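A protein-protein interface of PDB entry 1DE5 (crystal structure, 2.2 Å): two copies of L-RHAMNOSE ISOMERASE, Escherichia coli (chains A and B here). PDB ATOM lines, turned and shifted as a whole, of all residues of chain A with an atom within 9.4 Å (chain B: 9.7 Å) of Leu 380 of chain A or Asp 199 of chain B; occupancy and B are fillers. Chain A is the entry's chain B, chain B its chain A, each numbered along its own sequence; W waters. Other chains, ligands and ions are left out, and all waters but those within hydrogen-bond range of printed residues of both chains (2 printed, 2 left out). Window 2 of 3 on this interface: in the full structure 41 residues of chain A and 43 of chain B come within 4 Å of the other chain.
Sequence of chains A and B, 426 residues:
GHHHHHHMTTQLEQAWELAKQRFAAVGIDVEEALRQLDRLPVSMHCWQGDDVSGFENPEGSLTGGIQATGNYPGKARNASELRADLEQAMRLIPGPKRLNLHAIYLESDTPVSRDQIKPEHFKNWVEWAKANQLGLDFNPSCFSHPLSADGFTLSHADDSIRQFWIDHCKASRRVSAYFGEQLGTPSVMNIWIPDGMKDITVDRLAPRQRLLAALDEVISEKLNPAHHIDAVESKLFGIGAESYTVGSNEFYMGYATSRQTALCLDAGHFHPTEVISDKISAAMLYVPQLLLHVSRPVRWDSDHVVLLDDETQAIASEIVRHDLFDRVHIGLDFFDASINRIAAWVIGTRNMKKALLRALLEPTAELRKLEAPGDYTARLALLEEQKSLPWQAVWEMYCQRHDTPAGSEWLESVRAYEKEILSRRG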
ATOM      1  N   ARG A 321     -23.089  -2.910  -9.948  1.00  0.00           N
ATOM      2  CA  ARG A 321     -23.180  -1.461  -9.744  1.00  0.00           C
ATOM      3  C   ARG A 321     -24.067  -0.847 -10.825  1.00  0.00           C
ATOM      4  O   ARG A 321     -24.745   0.158 -10.699  1.00  0.00           O
ATOM      5  CB  ARG A 321     -21.795  -0.806  -9.850  1.00  0.00           C
ATOM      6  CG  ARG A 321     -20.914  -0.974  -8.610  1.00  0.00           C
ATOM      7  CD  ARG A 321     -19.467  -0.481  -8.756  1.00  0.00           C
ATOM      8  NE  ARG A 321     -18.849  -0.558  -7.426  1.00  0.00           N
ATOM      9  CZ  ARG A 321     -17.542  -0.500  -7.270  1.00  0.00           C
ATOM     10  NH1 ARG A 321     -16.800  -0.355  -8.310  1.00  0.00           N
ATOM     11  NH2 ARG A 321     -16.945  -0.560  -6.086  1.00  0.00           N
ATOM     12  N   LEU A 367     -21.951   5.343  -1.965  1.00  0.00           N
ATOM     13  CA  LEU A 367     -20.602   5.476  -2.426  1.00  0.00           C
ATOM     14  C   LEU A 367     -20.532   6.336  -3.667  1.00  0.00           C
ATOM     15  O   LEU A 367     -19.648   7.174  -3.850  1.00  0.00           O
ATOM     16  CB  LEU A 367     -19.912   4.095  -2.616  1.00  0.00           C
ATOM     17  CG  LEU A 367     -19.799   3.289  -1.335  1.00  0.00           C
ATOM     18  CD1 LEU A 367     -19.058   2.002  -1.671  1.00  0.00           C
ATOM     19  CD2 LEU A 367     -18.921   4.143  -0.409  1.00  0.00           C
ATOM     20  N   LEU A 370     -21.026   9.759  -2.547  1.00  0.00           N
ATOM     21  CA  LEU A 370     -19.840  10.425  -2.077  1.00  0.00           C
ATOM     22  C   LEU A 370     -18.897  10.754  -3.206  1.00  0.00           C
ATOM     23  O   LEU A 370     -18.097  11.721  -3.242  1.00  0.00           O
ATOM     24  CB  LEU A 370     -19.047   9.452  -1.171  1.00  0.00           C
ATOM     25  CG  LEU A 370     -19.642   9.330   0.220  1.00  0.00           C
ATOM     26  CD1 LEU A 370     -18.890   8.214   0.940  1.00  0.00           C
ATOM     27  CD2 LEU A 370     -19.441  10.645   1.004  1.00  0.00           C
ATOM     28  N   GLU A 371     -18.897   9.839  -4.114  1.00  0.00           N
ATOM     29  CA  GLU A 371     -17.921  10.032  -5.152  1.00  0.00           C
ATOM     30  C   GLU A 371     -18.211  11.226  -6.024  1.00  0.00           C
ATOM     31  O   GLU A 371     -17.338  11.995  -6.406  1.00  0.00           O
ATOM     32  CB  GLU A 371     -17.764   8.757  -5.985  1.00  0.00           C
ATOM     33  CG  GLU A 371     -17.010   9.047  -7.289  1.00  0.00           C
ATOM     34  CD  GLU A 371     -16.797   7.747  -8.018  1.00  0.00           C
ATOM     35  OE1 GLU A 371     -17.668   7.272  -8.730  1.00  0.00           O
ATOM     36  OE2 GLU A 371     -15.639   7.166  -7.728  1.00  0.00           O
ATOM     37  N   GLY A 374     -16.685  14.434  -4.839  1.00  0.00           N
ATOM     38  CA  GLY A 374     -15.280  14.680  -4.593  1.00  0.00           C
ATOM     39  C   GLY A 374     -14.851  14.218  -3.222  1.00  0.00           C
ATOM     40  O   GLY A 374     -13.683  14.378  -2.878  1.00  0.00           O
ATOM     41  N   ASP A 375     -15.790  13.580  -2.479  1.00  0.00           N
ATOM     42  CA  ASP A 375     -15.440  13.019  -1.194  1.00  0.00           C
ATOM     43  C   ASP A 375     -14.632  11.718  -1.355  1.00  0.00           C
ATOM     44  O   ASP A 375     -15.029  10.631  -0.895  1.00  0.00           O
ATOM     45  CB  ASP A 375     -16.591  12.866  -0.177  1.00  0.00           C
ATOM     46  CG  ASP A 375     -16.005  12.643   1.215  1.00  0.00           C
ATOM     47  OD1 ASP A 375     -14.823  12.396   1.377  1.00  0.00           O
ATOM     48  OD2 ASP A 375     -16.846  12.700   2.230  1.00  0.00           O
ATOM     49  N   TYR A 376     -13.478  11.846  -2.007  1.00  0.00           N
ATOM     50  CA  TYR A 376     -12.586  10.710  -2.278  1.00  0.00           C
ATOM     51  C   TYR A 376     -11.991  10.124  -1.001  1.00  0.00           C
ATOM     52  O   TYR A 376     -11.512   8.995  -0.966  1.00  0.00           O
ATOM     53  CB  TYR A 376     -11.457  11.090  -3.289  1.00  0.00           C
ATOM     54  CG  TYR A 376     -11.946  11.594  -4.664  1.00  0.00           C
ATOM     55  CD1 TYR A 376     -11.102  12.263  -5.551  1.00  0.00           C
ATOM     56  CD2 TYR A 376     -13.278  11.407  -5.038  1.00  0.00           C
ATOM     57  CE1 TYR A 376     -11.570  12.724  -6.786  1.00  0.00           C
ATOM     58  CE2 TYR A 376     -13.783  11.868  -6.249  1.00  0.00           C
ATOM     59  CZ  TYR A 376     -12.907  12.509  -7.123  1.00  0.00           C
ATOM     60  OH  TYR A 376     -13.403  12.904  -8.330  1.00  0.00           O
ATOM     61  N   THR A 377     -11.974  10.912   0.072  1.00  0.00           N
ATOM     62  CA  THR A 377     -11.432  10.387   1.298  1.00  0.00           C
ATOM     63  C   THR A 377     -12.396   9.333   1.754  1.00  0.00           C
ATOM     64  O   THR A 377     -12.059   8.179   1.929  1.00  0.00           O
ATOM     65  CB  THR A 377     -11.249  11.489   2.353  1.00  0.00           C
ATOM     66  OG1 THR A 377     -10.403  12.540   1.850  1.00  0.00           O
ATOM     67  CG2 THR A 377     -10.679  10.897   3.649  1.00  0.00           C
ATOM     68  N   ALA A 378     -13.641   9.730   1.873  1.00  0.00           N
ATOM     69  CA  ALA A 378     -14.666   8.821   2.318  1.00  0.00           C
ATOM     70  C   ALA A 378     -14.922   7.698   1.327  1.00  0.00           C
ATOM     71  O   ALA A 378     -15.263   6.609   1.717  1.00  0.00           O
ATOM     72  CB  ALA A 378     -15.927   9.568   2.677  1.00  0.00           C
ATOM     73  N   ARG A 379     -14.762   7.945   0.036  1.00  0.00           N
ATOM     74  CA  ARG A 379     -14.995   6.863  -0.947  1.00  0.00           C
ATOM     75  C   ARG A 379     -14.050   5.688  -0.633  1.00  0.00           C
ATOM     76  O   ARG A 379     -14.466   4.544  -0.435  1.00  0.00           O
ATOM     77  CB  ARG A 379     -14.629   7.350  -2.334  1.00  0.00           C
ATOM     78  CG  ARG A 379     -15.024   6.411  -3.473  1.00  0.00           C
ATOM     79  CD  ARG A 379     -14.460   6.877  -4.841  1.00  0.00           C
ATOM     80  NE  ARG A 379     -13.055   7.318  -4.834  1.00  0.00           N
ATOM     81  CZ  ARG A 379     -12.560   7.998  -5.868  1.00  0.00           C
ATOM     82  NH1 ARG A 379     -13.291   8.296  -6.940  1.00  0.00           N
ATOM     83  NH2 ARG A 379     -11.312   8.398  -5.867  1.00  0.00           N
ATOM     84  N   LEU A 380     -12.740   6.010  -0.622  1.00  0.00           N
ATOM     85  CA  LEU A 380     -11.702   5.040  -0.361  1.00  0.00           C
ATOM     86  C   LEU A 380     -11.840   4.319   1.002  1.00  0.00           C
ATOM     87  O   LEU A 380     -11.590   3.120   1.220  1.00  0.00           O
ATOM     88  CB  LEU A 380     -10.352   5.717  -0.459  1.00  0.00           C
ATOM     89  CG  LEU A 380      -9.225   4.692  -0.409  1.00  0.00           C
ATOM     90  CD1 LEU A 380      -9.321   3.759  -1.627  1.00  0.00           C
ATOM     91  CD2 LEU A 380      -7.898   5.436  -0.465  1.00  0.00           C
ATOM     92  N   ALA A 381     -12.244   5.090   1.967  1.00  0.00           N
ATOM     93  CA  ALA A 381     -12.391   4.591   3.307  1.00  0.00           C
ATOM     94  C   ALA A 381     -13.500   3.582   3.413  1.00  0.00           C
ATOM     95  O   ALA A 381     -13.336   2.472   3.948  1.00  0.00           O
ATOM     96  CB  ALA A 381     -12.595   5.774   4.235  1.00  0.00           C
ATOM     97  N   LEU A 382     -14.640   3.999   2.898  1.00  0.00           N
ATOM     98  CA  LEU A 382     -15.800   3.163   2.920  1.00  0.00           C
ATOM     99  C   LEU A 382     -15.624   1.974   2.048  1.00  0.00           C
ATOM    100  O   LEU A 382     -16.090   0.915   2.378  1.00  0.00           O
ATOM    101  CB  LEU A 382     -17.015   3.897   2.441  1.00  0.00           C
ATOM    102  CG  LEU A 382     -17.482   4.858   3.507  1.00  0.00           C
ATOM    103  CD1 LEU A 382     -18.906   5.277   3.187  1.00  0.00           C
ATOM    104  CD2 LEU A 382     -17.416   4.210   4.889  1.00  0.00           C
ATOM    105  N   LEU A 383     -14.990   2.189   0.928  1.00  0.00           N
ATOM    106  CA  LEU A 383     -14.748   1.103   0.038  1.00  0.00           C
ATOM    107  C   LEU A 383     -13.973   0.037   0.808  1.00  0.00           C
ATOM    108  O   LEU A 383     -14.281  -1.162   0.849  1.00  0.00           O
ATOM    109  CB  LEU A 383     -13.903   1.590  -1.139  1.00  0.00           C
ATOM    110  CG  LEU A 383     -14.707   2.226  -2.315  1.00  0.00           C
ATOM    111  CD1 LEU A 383     -13.755   2.741  -3.389  1.00  0.00           C
ATOM    112  CD2 LEU A 383     -15.593   1.211  -3.028  1.00  0.00           C
ATOM    113  N   GLU A 384     -12.917   0.518   1.431  1.00  0.00           N
ATOM    114  CA  GLU A 384     -12.052  -0.304   2.208  1.00  0.00           C
ATOM    115  C   GLU A 384     -12.742  -0.845   3.418  1.00  0.00           C
ATOM    116  O   GLU A 384     -12.511  -1.990   3.847  1.00  0.00           O
ATOM    117  CB  GLU A 384     -10.776   0.424   2.584  1.00  0.00           C
ATOM    118  CG  GLU A 384      -9.900   0.522   1.327  1.00  0.00           C
ATOM    119  CD  GLU A 384      -9.400  -0.817   0.823  1.00  0.00           C
ATOM    120  OE1 GLU A 384      -8.584  -1.495   1.419  1.00  0.00           O
ATOM    121  OE2 GLU A 384      -9.864  -1.134  -0.365  1.00  0.00           O
ATOM    122  N   GLU A 385     -13.614  -0.053   3.997  1.00  0.00           N
ATOM    123  CA  GLU A 385     -14.249  -0.614   5.174  1.00  0.00           C
ATOM    124  C   GLU A 385     -15.195  -1.710   4.763  1.00  0.00           C
ATOM    125  O   GLU A 385     -15.575  -2.565   5.577  1.00  0.00           O
ATOM    126  CB  GLU A 385     -14.987   0.400   6.085  1.00  0.00           C
ATOM    127  CG  GLU A 385     -14.079   1.262   6.979  1.00  0.00           C
ATOM    128  CD  GLU A 385     -13.196   0.431   7.842  1.00  0.00           C
ATOM    129  OE1 GLU A 385     -13.533  -0.647   8.301  1.00  0.00           O
ATOM    130  OE2 GLU A 385     -12.035   0.985   8.017  1.00  0.00           O
ATOM    131  N   GLN A 386     -15.571  -1.704   3.487  1.00  0.00           N
ATOM    132  CA  GLN A 386     -16.535  -2.714   3.054  1.00  0.00           C
ATOM    133  C   GLN A 386     -15.946  -4.085   3.255  1.00  0.00           C
ATOM    134  O   GLN A 386     -16.629  -4.987   3.650  1.00  0.00           O
ATOM    135  CB  GLN A 386     -16.827  -2.627   1.544  1.00  0.00           C
ATOM    136  CG  GLN A 386     -17.885  -1.620   1.114  1.00  0.00           C
ATOM    137  CD  GLN A 386     -18.934  -1.533   2.161  1.00  0.00           C
ATOM    138  OE1 GLN A 386     -18.744  -0.745   3.121  1.00  0.00           O
ATOM    139  NE2 GLN A 386     -19.973  -2.371   1.968  1.00  0.00           N
ATOM    140  N   LYS A 387     -14.667  -4.179   2.935  1.00  0.00           N
ATOM    141  CA  LYS A 387     -13.938  -5.432   3.030  1.00  0.00           C
ATOM    142  C   LYS A 387     -14.060  -6.071   4.405  1.00  0.00           C
ATOM    143  O   LYS A 387     -13.891  -7.283   4.534  1.00  0.00           O
ATOM    144  CB  LYS A 387     -12.493  -5.255   2.571  1.00  0.00           C
ATOM    145  CG  LYS A 387     -12.492  -4.698   1.125  1.00  0.00           C
ATOM    146  CD  LYS A 387     -11.079  -4.503   0.584  1.00  0.00           C
ATOM    147  CE  LYS A 387     -10.940  -3.967  -0.858  1.00  0.00           C
ATOM    148  NZ  LYS A 387      -9.501  -3.728  -1.221  1.00  0.00           N
ATOM    149  N   PHE B 152     -12.057  16.382 -14.639  1.00  0.00           N
ATOM    150  CA  PHE B 152     -13.064  16.048 -15.655  1.00  0.00           C
ATOM    151  C   PHE B 152     -13.354  17.201 -16.599  1.00  0.00           C
ATOM    152  O   PHE B 152     -13.240  18.331 -16.193  1.00  0.00           O
ATOM    153  CB  PHE B 152     -14.375  15.515 -15.097  1.00  0.00           C
ATOM    154  CG  PHE B 152     -13.977  14.327 -14.287  1.00  0.00           C
ATOM    155  CD1 PHE B 152     -13.717  14.483 -12.926  1.00  0.00           C
ATOM    156  CD2 PHE B 152     -13.783  13.080 -14.883  1.00  0.00           C
ATOM    157  CE1 PHE B 152     -13.346  13.384 -12.155  1.00  0.00           C
ATOM    158  CE2 PHE B 152     -13.380  11.983 -14.123  1.00  0.00           C
ATOM    159  CZ  PHE B 152     -13.150  12.145 -12.761  1.00  0.00           C
ATOM    160  N   GLY B 196     -10.416  11.314 -16.015  1.00  0.00           N
ATOM    161  CA  GLY B 196     -10.160  10.053 -15.349  1.00  0.00           C
ATOM    162  C   GLY B 196     -10.057  10.265 -13.858  1.00  0.00           C
ATOM    163  O   GLY B 196     -10.217  11.380 -13.422  1.00  0.00           O
ATOM    164  N   MET B 197      -9.826   9.192 -13.082  1.00  0.00           N
ATOM    165  CA  MET B 197      -9.633   9.230 -11.626  1.00  0.00           C
ATOM    166  C   MET B 197      -8.282   8.736 -11.196  1.00  0.00           C
ATOM    167  O   MET B 197      -7.744   7.770 -11.740  1.00  0.00           O
ATOM    168  CB  MET B 197     -10.635   8.414 -10.825  1.00  0.00           C
ATOM    169  CG  MET B 197     -12.004   8.991 -11.012  1.00  0.00           C
ATOM    170  SD  MET B 197     -12.363   9.963  -9.563  1.00  0.00           S
ATOM    171  CE  MET B 197     -14.142  10.044  -9.788  1.00  0.00           C
ATOM    172  N   LYS B 198      -7.776   9.347 -10.142  1.00  0.00           N
ATOM    173  CA  LYS B 198      -6.490   8.923  -9.607  1.00  0.00           C
ATOM    174  C   LYS B 198      -6.592   7.561  -8.908  1.00  0.00           C
ATOM    175  O   LYS B 198      -5.691   6.728  -8.979  1.00  0.00           O
ATOM    176  CB  LYS B 198      -6.047   9.931  -8.540  1.00  0.00           C
ATOM    177  CG  LYS B 198      -4.616   9.705  -8.069  1.00  0.00           C
ATOM    178  CD  LYS B 198      -4.253  10.412  -6.767  1.00  0.00           C
ATOM    179  CE  LYS B 198      -2.787  10.191  -6.349  1.00  0.00           C
ATOM    180  NZ  LYS B 198      -2.268  11.024  -5.231  1.00  0.00           N
ATOM    181  N   ASP B 199      -7.702   7.352  -8.200  1.00  0.00           N
ATOM    182  CA  ASP B 199      -7.829   6.158  -7.397  1.00  0.00           C
ATOM    183  C   ASP B 199      -9.053   5.310  -7.635  1.00  0.00           C
ATOM    184  O   ASP B 199      -9.822   5.568  -8.539  1.00  0.00           O
ATOM    185  CB  ASP B 199      -7.725   6.563  -5.895  1.00  0.00           C
ATOM    186  CG  ASP B 199      -6.958   5.515  -5.144  1.00  0.00           C
ATOM    187  OD1 ASP B 199      -6.835   4.377  -5.522  1.00  0.00           O
ATOM    188  OD2 ASP B 199      -6.498   5.929  -4.013  1.00  0.00           O
ATOM    189  N   ILE B 200      -9.223   4.290  -6.802  1.00  0.00           N
ATOM    190  CA  ILE B 200     -10.386   3.397  -6.927  1.00  0.00           C
ATOM    191  C   ILE B 200     -11.689   4.142  -7.178  1.00  0.00           C
ATOM    192  O   ILE B 200     -12.161   5.017  -6.432  1.00  0.00           O
ATOM    193  CB  ILE B 200     -10.499   2.421  -5.757  1.00  0.00           C
ATOM    194  CG1 ILE B 200      -9.108   1.916  -5.356  1.00  0.00           C
ATOM    195  CG2 ILE B 200     -11.469   1.280  -6.088  1.00  0.00           C
ATOM    196  CD1 ILE B 200      -8.455   1.000  -6.379  1.00  0.00           C
ATOM    197  N   THR B 201     -12.315   3.767  -8.274  1.00  0.00           N
ATOM    198  CA  THR B 201     -13.543   4.382  -8.753  1.00  0.00           C
ATOM    199  C   THR B 201     -14.809   3.548  -8.637  1.00  0.00           C
ATOM    200  O   THR B 201     -14.880   2.399  -9.038  1.00  0.00           O
ATOM    201  CB  THR B 201     -13.269   4.647 -10.258  1.00  0.00           C
ATOM    202  OG1 THR B 201     -12.129   5.471 -10.383  1.00  0.00           O
ATOM    203  CG2 THR B 201     -14.434   5.246 -11.047  1.00  0.00           C
ATOM    204  N   VAL B 202     -15.876   4.175  -8.186  1.00  0.00           N
ATOM    205  CA  VAL B 202     -17.159   3.540  -8.116  1.00  0.00           C
ATOM    206  C   VAL B 202     -17.937   3.560  -9.422  1.00  0.00           C
ATOM    207  O   VAL B 202     -18.536   2.580  -9.812  1.00  0.00           O
ATOM    208  CB  VAL B 202     -18.033   4.249  -7.097  1.00  0.00           C
ATOM    209  CG1 VAL B 202     -19.355   3.522  -6.863  1.00  0.00           C
ATOM    210  CG2 VAL B 202     -17.257   4.296  -5.812  1.00  0.00           C
ATOM    211  N   ASP B 203     -18.050   4.708 -10.056  1.00  0.00           N
ATOM    212  CA  ASP B 203     -18.895   4.738 -11.211  1.00  0.00           C
ATOM    213  C   ASP B 203     -18.183   5.107 -12.470  1.00  0.00           C
ATOM    214  O   ASP B 203     -18.064   6.278 -12.832  1.00  0.00           O
ATOM    215  CB  ASP B 203     -20.096   5.688 -11.045  1.00  0.00           C
ATOM    216  CG  ASP B 203     -20.997   5.598 -12.272  1.00  0.00           C
ATOM    217  OD1 ASP B 203     -20.828   4.906 -13.286  1.00  0.00           O
ATOM    218  OD2 ASP B 203     -22.087   6.244 -12.040  1.00  0.00           O
ATOM    219  N   ARG B 204     -17.764   4.069 -13.137  1.00  0.00           N
ATOM    220  CA  ARG B 204     -17.094   4.183 -14.401  1.00  0.00           C
ATOM    221  C   ARG B 204     -18.089   4.408 -15.550  1.00  0.00           C
ATOM    222  O   ARG B 204     -17.643   4.665 -16.665  1.00  0.00           O
ATOM    223  CB  ARG B 204     -16.312   2.883 -14.674  1.00  0.00           C
ATOM    224  CG  ARG B 204     -15.030   2.855 -13.881  1.00  0.00           C
ATOM    225  CD  ARG B 204     -14.385   1.499 -13.789  1.00  0.00           C
ATOM    226  NE  ARG B 204     -13.057   1.569 -14.313  1.00  0.00           N
ATOM    227  CZ  ARG B 204     -11.906   1.628 -13.652  1.00  0.00           C
ATOM    228  NH1 ARG B 204     -11.776   1.601 -12.344  1.00  0.00           N
ATOM    229  NH2 ARG B 204     -10.790   1.700 -14.380  1.00  0.00           N
ATOM    230  N   PHE B 237      -3.796   5.635 -18.813  1.00  0.00           N
ATOM    231  CA  PHE B 237      -3.649   6.284 -17.512  1.00  0.00           C
ATOM    232  C   PHE B 237      -2.696   7.479 -17.565  1.00  0.00           C
ATOM    233  O   PHE B 237      -1.727   7.535 -18.356  1.00  0.00           O
ATOM    234  CB  PHE B 237      -3.092   5.298 -16.449  1.00  0.00           C
ATOM    235  CG  PHE B 237      -1.591   5.131 -16.543  1.00  0.00           C
ATOM    236  CD1 PHE B 237      -0.757   5.798 -15.632  1.00  0.00           C
ATOM    237  CD2 PHE B 237      -1.018   4.347 -17.550  1.00  0.00           C
ATOM    238  CE1 PHE B 237       0.630   5.648 -15.682  1.00  0.00           C
ATOM    239  CE2 PHE B 237       0.371   4.229 -17.655  1.00  0.00           C
ATOM    240  CZ  PHE B 237       1.180   4.873 -16.708  1.00  0.00           C
ATOM    241  N   GLY B 238      -2.967   8.410 -16.659  1.00  0.00           N
ATOM    242  CA  GLY B 238      -2.181   9.629 -16.506  1.00  0.00           C
ATOM    243  C   GLY B 238      -1.731   9.830 -15.063  1.00  0.00           C
ATOM    244  O   GLY B 238      -2.314   9.252 -14.121  1.00  0.00           O
ATOM    245  N   ILE B 239      -0.677  10.649 -14.902  1.00  0.00           N
ATOM    246  CA  ILE B 239      -0.149  10.916 -13.577  1.00  0.00           C
ATOM    247  C   ILE B 239      -1.195  11.698 -12.812  1.00  0.00           C
ATOM    248  O   ILE B 239      -1.615  12.734 -13.290  1.00  0.00           O
ATOM    249  CB  ILE B 239       1.224  11.563 -13.578  1.00  0.00           C
ATOM    250  CG1 ILE B 239       2.252  10.660 -14.305  1.00  0.00           C
ATOM    251  CG2 ILE B 239       1.636  11.729 -12.116  1.00  0.00           C
ATOM    252  CD1 ILE B 239       3.694  11.005 -13.918  1.00  0.00           C
ATOM    253  N   GLY B 240      -1.663  11.158 -11.682  1.00  0.00           N
ATOM    254  CA  GLY B 240      -2.739  11.796 -10.919  1.00  0.00           C
ATOM    255  C   GLY B 240      -4.102  11.293 -11.435  1.00  0.00           C
ATOM    256  O   GLY B 240      -5.208  11.575 -10.933  1.00  0.00           O
ATOM    257  N   ALA B 241      -4.042  10.507 -12.489  1.00  0.00           N
ATOM    258  CA  ALA B 241      -5.258   9.934 -13.076  1.00  0.00           C
ATOM    259  C   ALA B 241      -4.963   8.489 -13.496  1.00  0.00           C
ATOM    260  O   ALA B 241      -5.405   8.017 -14.526  1.00  0.00           O
ATOM    261  CB  ALA B 241      -5.798  10.747 -14.272  1.00  0.00           C
ATOM    262  N   GLU B 242      -4.189   7.805 -12.659  1.00  0.00           N
ATOM    263  CA  GLU B 242      -3.759   6.449 -12.875  1.00  0.00           C
ATOM    264  C   GLU B 242      -4.823   5.371 -12.893  1.00  0.00           C
ATOM    265  O   GLU B 242      -4.631   4.354 -13.495  1.00  0.00           O
ATOM    266  CB  GLU B 242      -2.799   6.106 -11.736  1.00  0.00           C
ATOM    267  CG  GLU B 242      -1.539   6.991 -11.778  1.00  0.00           C
ATOM    268  CD  GLU B 242      -1.625   8.187 -10.861  1.00  0.00           C
ATOM    269  OE1 GLU B 242      -0.649   8.843 -10.571  1.00  0.00           O
ATOM    270  OE2 GLU B 242      -2.834   8.452 -10.378  1.00  0.00           O
ATOM    271  N   SER B 243      -5.935   5.539 -12.249  1.00  0.00           N
ATOM    272  CA  SER B 243      -6.784   4.389 -12.130  1.00  0.00           C
ATOM    273  C   SER B 243      -7.927   4.136 -13.040  1.00  0.00           C
ATOM    274  O   SER B 243      -8.441   3.019 -13.200  1.00  0.00           O
ATOM    275  CB  SER B 243      -6.837   3.848 -10.681  1.00  0.00           C
ATOM    276  OG  SER B 243      -7.981   4.193  -9.959  1.00  0.00           O
ATOM    277  N   TYR B 244      -8.335   5.212 -13.627  1.00  0.00           N
ATOM    278  CA  TYR B 244      -9.443   5.122 -14.529  1.00  0.00           C
ATOM    279  C   TYR B 244      -9.379   6.218 -15.572  1.00  0.00           C
ATOM    280  O   TYR B 244      -9.058   7.338 -15.226  1.00  0.00           O
ATOM    281  CB  TYR B 244     -10.696   5.230 -13.696  1.00  0.00           C
ATOM    282  CG  TYR B 244     -11.950   5.689 -14.408  1.00  0.00           C
ATOM    283  CD1 TYR B 244     -12.538   4.943 -15.425  1.00  0.00           C
ATOM    284  CD2 TYR B 244     -12.630   6.826 -13.987  1.00  0.00           C
ATOM    285  CE1 TYR B 244     -13.696   5.344 -16.083  1.00  0.00           C
ATOM    286  CE2 TYR B 244     -13.832   7.210 -14.590  1.00  0.00           C
ATOM    287  CZ  TYR B 244     -14.371   6.476 -15.646  1.00  0.00           C
ATOM    288  OH  TYR B 244     -15.577   6.833 -16.228  1.00  0.00           O
ATOM    289  N   THR B 245      -9.617   5.860 -16.829  1.00  0.00           N
ATOM    290  CA  THR B 245      -9.646   6.795 -17.932  1.00  0.00           C
ATOM    291  C   THR B 245     -10.988   6.684 -18.590  1.00  0.00           C
ATOM    292  O   THR B 245     -11.305   5.613 -19.081  1.00  0.00           O
ATOM    293  CB  THR B 245      -8.596   6.567 -19.007  1.00  0.00           C
ATOM    294  OG1 THR B 245      -7.361   6.429 -18.377  1.00  0.00           O
ATOM    295  CG2 THR B 245      -8.579   7.720 -20.029  1.00  0.00           C
HETATM  296  O   HOH W   1     -11.484   5.540  -3.828  1.00  0.00           O
HETATM  297  O   HOH W   2     -17.338   8.414 -11.438  1.00  0.00           O
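SD of Met 197 of chain B lies close to OH of Tyr 376 of chain A (3.4 Å). SD of Met 197 of chain B lies within hydrogen-bond range of NH1 of Arg 379 of chain A (3.2 Å). NE of Arg 379 of chain A is in hydrogen-bond range of O of Ile 200 of chain B, at 2.9 Å. The backbone carbonyl oxygen of Thr 201 of chain B lies within hydrogen-bond range of the guanidinium group of Arg 321 of chain A (3.4 Å). The backbone NH (N) of Val 202 of chain B sits at hydrogen-bond distance from the side-chain carboxylate (OE2) of Glu 371 of chain A, at 3.0 Å. The side-chain carboxylate (OE1) of Glu 371 of chain A is in hydrogen-bond range of the backbone NH (N) of Asp 203 of chain B, at 2.9 Å.
The backbone NH (N) of Met 197 of chain B is in hydrogen-bond range of the backbone carbonyl oxygen (O) of Tyr 244 of chain B, at 2.9 Å. The backbone carbonyl oxygen (O) of Asp 199 of chain B is in hydrogen-bond range of the side-chain hydroxyl (OG) of Ser 243 of chain B (2.7 Å). The guanidinium group of Arg 379 of chain A lies within salt-bridge range of the side-chain carboxylate of Glu 371 of chain A, 2.7 Å away.
Among the printed residues, pairs that only touch across the chains: Arg 321 of chain A with Val 202 of chain B, Glu 371 of chain A with Thr 201 of chain B, Leu 383 of chain A with Ile 200 of chain B, Glu 371 of chain A with Met 197 of chain B, Leu 380 of chain A with Asp 199 of chain B, Tyr 376 of chain A with Phe 152 of chain B and Arg 379 of chain A with Val 202 of chain B.
Leu 380 of chain A touches just one residue of chain B: Asp 199 (3.8 Å). Of chain A, only Leu 380 (3.8 Å) comes within 4 Å of Asp 199 of chain B. No residue of chain B comes within 4 Å of Ala 381 of chain A. Of chain A, only Arg 379 (2.9 Å) and Leu 383 (3.8 Å) come within 4 Å of Ile 200 of chain B. Of the printed residues of chain B, Glu 371 of chain A touches Met 197, Thr 201, Val 202 and Asp 203. Printed residues of chain A within 4 Å of Val 202 of chain B: Arg 321, Glu 371 and Arg 379. Of the printed residues of chain B, Leu 383 of chain A touches Ile 200. Printed residues of chain A within 4 Å of Met 197 of chain B: Glu 371, Tyr 376 and Arg 379. The nearest residue of chain B that does not touch Leu 380 of chain A is Ile 200 of chain B (4.2 Å). The nearest residue of chain A that does not touch Asp 199 of chain B is Arg 379 of chain A (4.03 Å). The nearest printed residue of chain B that does not touch Tyr 376 of chain A is Lys 198 of chain B (6.1 Å).
Printed residues of chain A that touch a printed residue of chain B: Arg 321, Glu 371, Tyr 376, Arg 379, Leu 380 and Leu 383. Hydrophobic or aromatic side chains of chain A within 4 Å of the printed part of chain B: Tyr 376, Leu 380 and Leu 383.
No position is printed for both chains. Of the 13 pairs that touch across the chains among the printed residues, none has its exchanged pair printed and touching as well.
Water W1 lies within hydrogen-bond range of NE of Arg 379 of chain A (2.6 Å), O of Ile 200 of chain B (2.7 Å) and N of Leu 380 of chain A (3.5 Å). Water W2 bridges O of Asp 203 of chain B (2.7 Å) and OE1 of Glu 371 of chain A (3.0 Å).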
